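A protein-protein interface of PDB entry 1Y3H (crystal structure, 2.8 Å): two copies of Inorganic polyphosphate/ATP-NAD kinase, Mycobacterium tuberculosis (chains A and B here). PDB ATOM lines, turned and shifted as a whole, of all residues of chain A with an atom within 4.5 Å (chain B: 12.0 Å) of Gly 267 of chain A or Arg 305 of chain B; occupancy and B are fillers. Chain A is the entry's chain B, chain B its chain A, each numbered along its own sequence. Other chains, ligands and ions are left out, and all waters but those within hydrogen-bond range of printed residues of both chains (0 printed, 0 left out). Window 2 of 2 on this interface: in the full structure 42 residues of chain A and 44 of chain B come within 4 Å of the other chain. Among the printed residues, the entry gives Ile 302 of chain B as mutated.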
ATOM      1  N   GLU A 244     -17.240  25.145  23.787  1.00  0.00           N
ATOM      2  CA  GLU A 244     -17.485  25.392  25.206  1.00  0.00           C
ATOM      3  C   GLU A 244     -16.200  25.279  26.011  1.00  0.00           C
ATOM      4  O   GLU A 244     -15.502  24.267  25.942  1.00  0.00           O
ATOM      5  CB  GLU A 244     -18.529  24.400  25.734  1.00  0.00           C
ATOM      6  CG  GLU A 244     -19.925  24.627  25.150  1.00  0.00           C
ATOM      7  CD  GLU A 244     -20.943  23.581  25.573  1.00  0.00           C
ATOM      8  OE1 GLU A 244     -22.155  23.830  25.382  1.00  0.00           O
ATOM      9  OE2 GLU A 244     -20.536  22.514  26.087  1.00  0.00           O
ATOM     10  N   ILE A 245     -15.882  26.337  26.755  1.00  0.00           N
ATOM     11  CA  ILE A 245     -14.683  26.370  27.591  1.00  0.00           C
ATOM     12  C   ILE A 245     -15.016  25.951  29.019  1.00  0.00           C
ATOM     13  O   ILE A 245     -16.030  26.359  29.588  1.00  0.00           O
ATOM     14  CB  ILE A 245     -14.027  27.786  27.620  1.00  0.00           C
ATOM     15  CG1 ILE A 245     -13.182  28.005  26.363  1.00  0.00           C
ATOM     16  CG2 ILE A 245     -13.133  27.935  28.836  1.00  0.00           C
ATOM     17  CD1 ILE A 245     -13.996  28.212  25.091  1.00  0.00           C
ATOM     18  N   GLU A 246     -14.145  25.126  29.582  1.00  0.00           N
ATOM     19  CA  GLU A 246     -14.288  24.610  30.937  1.00  0.00           C
ATOM     20  C   GLU A 246     -14.548  25.689  31.983  1.00  0.00           C
ATOM     21  O   GLU A 246     -13.748  26.607  32.142  1.00  0.00           O
ATOM     22  CB  GLU A 246     -13.023  23.844  31.297  1.00  0.00           C
ATOM     23  CG  GLU A 246     -12.883  23.450  32.742  1.00  0.00           C
ATOM     24  CD  GLU A 246     -11.549  22.783  32.992  1.00  0.00           C
ATOM     25  OE1 GLU A 246     -10.509  23.378  32.612  1.00  0.00           O
ATOM     26  OE2 GLU A 246     -11.539  21.672  33.568  1.00  0.00           O
ATOM     27  N   ALA A 247     -15.661  25.553  32.699  1.00  0.00           N
ATOM     28  CA  ALA A 247     -16.041  26.507  33.743  1.00  0.00           C
ATOM     29  C   ALA A 247     -15.025  26.516  34.872  1.00  0.00           C
ATOM     30  O   ALA A 247     -14.542  27.565  35.284  1.00  0.00           O
ATOM     31  CB  ALA A 247     -17.411  26.154  34.293  1.00  0.00           C
ATOM     32  N   PRO A 265     -13.983  34.423  29.012  1.00  0.00           N
ATOM     33  CA  PRO A 265     -14.226  34.078  30.415  1.00  0.00           C
ATOM     34  C   PRO A 265     -14.550  32.593  30.587  1.00  0.00           C
ATOM     35  O   PRO A 265     -15.433  32.055  29.914  1.00  0.00           O
ATOM     36  CB  PRO A 265     -15.406  34.969  30.775  1.00  0.00           C
ATOM     37  CG  PRO A 265     -16.198  34.964  29.503  1.00  0.00           C
ATOM     38  CD  PRO A 265     -15.123  35.180  28.459  1.00  0.00           C
ATOM     39  N   ALA A 266     -13.834  31.931  31.489  1.00  0.00           N
ATOM     40  CA  ALA A 266     -14.070  30.519  31.737  1.00  0.00           C
ATOM     41  C   ALA A 266     -15.561  30.246  31.725  1.00  0.00           C
ATOM     42  O   ALA A 266     -16.354  31.079  32.148  1.00  0.00           O
ATOM     43  CB  ALA A 266     -13.480  30.121  33.075  1.00  0.00           C
ATOM     44  N   GLY A 267     -15.948  29.087  31.218  1.00  0.00           N
ATOM     45  CA  GLY A 267     -17.356  28.751  31.195  1.00  0.00           C
ATOM     46  C   GLY A 267     -18.170  29.446  30.128  1.00  0.00           C
ATOM     47  O   GLY A 267     -19.392  29.292  30.092  1.00  0.00           O
ATOM     48  N   SER A 268     -17.519  30.228  29.271  1.00  0.00           N
ATOM     49  CA  SER A 268     -18.239  30.902  28.185  1.00  0.00           C
ATOM     50  C   SER A 268     -18.046  30.055  26.937  1.00  0.00           C
ATOM     51  O   SER A 268     -17.053  29.322  26.835  1.00  0.00           O
ATOM     52  CB  SER A 268     -17.697  32.318  27.942  1.00  0.00           C
ATOM     53  OG  SER A 268     -16.348  32.297  27.514  1.00  0.00           O
ATOM     54  N   ARG A 269     -18.991  30.132  25.998  1.00  0.00           N
ATOM     55  CA  ARG A 269     -18.863  29.346  24.778  1.00  0.00           C
ATOM     56  C   ARG A 269     -18.729  30.152  23.492  1.00  0.00           C
ATOM     57  O   ARG A 269     -19.554  31.001  23.154  1.00  0.00           O
ATOM     58  CB  ARG A 269     -20.005  28.335  24.651  1.00  0.00           C
ATOM     59  CG  ARG A 269     -21.315  28.859  24.160  1.00  0.00           C
ATOM     60  CD  ARG A 269     -22.273  27.697  24.067  1.00  0.00           C
ATOM     61  NE  ARG A 269     -22.853  27.557  22.738  1.00  0.00           N
ATOM     62  CZ  ARG A 269     -23.350  26.421  22.259  1.00  0.00           C
ATOM     63  NH1 ARG A 269     -23.329  25.326  23.011  1.00  0.00           N
ATOM     64  NH2 ARG A 269     -23.869  26.375  21.035  1.00  0.00           N
ATOM     65  N   PRO B 300     -15.088  10.630  23.905  1.00  0.00           N
ATOM     66  CA  PRO B 300     -15.454  11.249  25.184  1.00  0.00           C
ATOM     67  C   PRO B 300     -16.139  12.596  24.985  1.00  0.00           C
ATOM     68  O   PRO B 300     -15.496  13.618  24.756  1.00  0.00           O
ATOM     69  CB  PRO B 300     -14.115  11.372  25.906  1.00  0.00           C
ATOM     70  CG  PRO B 300     -13.136  11.476  24.789  1.00  0.00           C
ATOM     71  CD  PRO B 300     -13.633  10.428  23.833  1.00  0.00           C
ATOM     72  N   VAL B 301     -17.458  12.569  25.083  1.00  0.00           N
ATOM     73  CA  VAL B 301     -18.279  13.746  24.905  1.00  0.00           C
ATOM     74  C   VAL B 301     -18.697  14.312  26.253  1.00  0.00           C
ATOM     75  O   VAL B 301     -19.573  15.168  26.329  1.00  0.00           O
ATOM     76  CB  VAL B 301     -19.522  13.368  24.077  1.00  0.00           C
ATOM     77  CG1 VAL B 301     -20.559  14.454  24.124  1.00  0.00           C
ATOM     78  CG2 VAL B 301     -19.109  13.099  22.650  1.00  0.00           C
ATOM     79  N   ILE B 302     -18.052  13.857  27.321  1.00  0.00           N
ATOM     80  CA  ILE B 302     -18.412  14.319  28.660  1.00  0.00           C
ATOM     81  C   ILE B 302     -17.958  15.715  29.066  1.00  0.00           C
ATOM     82  O   ILE B 302     -16.783  16.067  28.933  1.00  0.00           O
ATOM     83  CB  ILE B 302     -17.906  13.373  29.741  1.00  0.00           C
ATOM     84  CG1 ILE B 302     -18.579  13.749  31.060  1.00  0.00           C
ATOM     85  CG2 ILE B 302     -16.380  13.484  29.871  1.00  0.00           C
ATOM     86  CD1 ILE B 302     -20.090  13.944  30.930  1.00  0.00           C
ATOM     87  N   GLY B 303     -18.897  16.488  29.608  1.00  0.00           N
ATOM     88  CA  GLY B 303     -18.598  17.843  30.036  1.00  0.00           C
ATOM     89  C   GLY B 303     -19.355  18.851  29.194  1.00  0.00           C
ATOM     90  O   GLY B 303     -19.346  20.049  29.468  1.00  0.00           O
ATOM     91  N   TRP B 304     -20.021  18.353  28.161  1.00  0.00           N
ATOM     92  CA  TRP B 304     -20.789  19.199  27.261  1.00  0.00           C
ATOM     93  C   TRP B 304     -21.992  19.807  27.974  1.00  0.00           C
ATOM     94  O   TRP B 304     -22.658  19.135  28.758  1.00  0.00           O
ATOM     95  CB  TRP B 304     -21.260  18.369  26.063  1.00  0.00           C
ATOM     96  CG  TRP B 304     -22.037  19.143  25.059  1.00  0.00           C
ATOM     97  CD1 TRP B 304     -21.611  20.233  24.362  1.00  0.00           C
ATOM     98  CD2 TRP B 304     -23.388  18.897  24.642  1.00  0.00           C
ATOM     99  NE1 TRP B 304     -22.613  20.685  23.536  1.00  0.00           N
ATOM    100  CE2 TRP B 304     -23.714  19.883  23.688  1.00  0.00           C
ATOM    101  CE3 TRP B 304     -24.354  17.940  24.983  1.00  0.00           C
ATOM    102  CZ2 TRP B 304     -24.969  19.941  23.067  1.00  0.00           C
ATOM    103  CZ3 TRP B 304     -25.605  17.999  24.363  1.00  0.00           C
ATOM    104  CH2 TRP B 304     -25.897  18.993  23.419  1.00  0.00           C
ATOM    105  N   ARG B 305     -22.264  21.081  27.705  1.00  0.00           N
ATOM    106  CA  ARG B 305     -23.407  21.748  28.315  1.00  0.00           C
ATOM    107  C   ARG B 305     -24.504  21.870  27.265  1.00  0.00           C
ATOM    108  O   ARG B 305     -25.588  21.311  27.414  1.00  0.00           O
ATOM    109  CB  ARG B 305     -23.038  23.146  28.805  1.00  0.00           C
ATOM    110  CG  ARG B 305     -21.588  23.340  29.159  1.00  0.00           C
ATOM    111  CD  ARG B 305     -21.408  24.651  29.907  1.00  0.00           C
ATOM    112  NE  ARG B 305     -20.044  25.156  29.787  1.00  0.00           N
ATOM    113  CZ  ARG B 305     -19.571  25.824  28.740  1.00  0.00           C
ATOM    114  NH1 ARG B 305     -18.310  26.223  28.746  1.00  0.00           N
ATOM    115  NH2 ARG B 305     -20.355  26.111  27.705  1.00  0.00           N
ATOM    116  N   GLY B 306     -24.211  22.607  26.200  1.00  0.00           N
ATOM    117  CA  GLY B 306     -25.181  22.784  25.138  1.00  0.00           C
ATOM    118  C   GLY B 306     -25.638  24.222  25.035  1.00  0.00           C
ATOM    119  O   GLY B 306     -25.266  25.055  25.858  1.00  0.00           O
ATOM    120  N   LYS B 307     -26.448  24.508  24.019  1.00  0.00           N
ATOM    121  CA  LYS B 307     -26.977  25.851  23.774  1.00  0.00           C
ATOM    122  C   LYS B 307     -28.511  25.805  23.774  1.00  0.00           C
ATOM    123  O   LYS B 307     -29.123  26.127  22.728  1.00  0.00           O
ATOM    124  CB  LYS B 307     -26.462  26.376  22.424  1.00  0.00           C
ATOM    125  CG  LYS B 307     -26.868  27.806  22.071  1.00  0.00           C
ATOM    126  CD  LYS B 307     -26.384  28.178  20.669  1.00  0.00           C
ATOM    127  CE  LYS B 307     -26.963  29.504  20.188  1.00  0.00           C
ATOM    128  NZ  LYS B 307     -26.613  29.755  18.761  1.00  0.00           N
ATOM    129  OXT LYS B 307     -29.081  25.435  24.827  1.00  0.00           O
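NH2 of Arg 305 of chain B is in salt-bridge range of OE1 of Glu 244 of chain A (3.7 Å).
NH1 of Arg 305 of chain B sits at hydrogen-bond distance from O of Ile 245 of chain A, 2.4 Å away.
The backbone NH of Gly 306 of chain B sits at hydrogen-bond distance from the side-chain carboxylate of Glu 244 of chain A (2.5 Å).
O of Gly 306 of chain B sits close to NH1 of Arg 269 of chain A, at 3.5 Å.
The guanidinium group (NH1) of Arg 269 of chain A lies close to the backbone NH (N) of Lys 307 of chain B, at 3.4 Å.
The guanidinium group of Arg 269 of chain A is in salt-bridge range of the side-chain carboxylate of Glu 244 of chain A.
The backbone carbonyl oxygen of Ile 245 of chain A sits close to the backbone NH of Gly 267 of chain A, 3.2 Å away.
N of Ile 245 of chain A is in hydrogen-bond range of O of Ser 268 of chain A (3.2 Å).
O of Glu 246 of chain A sits at hydrogen-bond distance from N of Gly 267 of chain A, 3.4 Å away.
O of Pro 265 of chain A is in hydrogen-bond range of OG of Ser 268 of chain A.
Among the printed residues, pairs that only touch across the chains: Glu 244 of chain A with Trp 304 of chain B, Gly 267 of chain A with Arg 305 of chain B, Ser 268 of chain A with Arg 305 of chain B and Arg 269 of chain A with Arg 305 of chain B.
Of chain B, only Trp 304 (3.1 Å), Arg 305 (2.8 Å) and Gly 306 (2.5 Å) come within 4 Å of Glu 244 of chain A.
Ala 247 of chain A touches none of the printed residues of chain B.
Pro 265 of chain A touches none of the printed residues of chain B.
Gly 267 of chain A touches just one residue of chain B: Arg 305.
Pro 300 of chain B touches none of the printed residues of chain A.
Gly 303 of chain B touches none of the printed residues of chain A.
Of the printed residues of chain A, Trp 304 of chain B touches Glu 244 (3.1 Å).
Of the printed residues of chain A, Gly 306 of chain B touches Glu 244 (2.5 Å) and Arg 269 (3.3 Å).
Of the printed residues of chain A, Lys 307 of chain B touches Arg 269.
Printed residues of chain A that touch a printed residue of chain B: Glu 244, Ile 245, Gly 267, Ser 268 and Arg 269.
Hydrophobic or aromatic side chains of chain B that line the printed part of chain A: Trp 304.
Among the printed residues, Asp or Glu carboxylates within 4 Å of a Lys or Arg side-chain nitrogen of the other chain: Glu 244 of chain A with Arg 305 of chain B.
No position is printed for both chains.
Of the 9 pairs that touch across the chains among the printed residues, none has its exchanged pair printed and touching as well.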
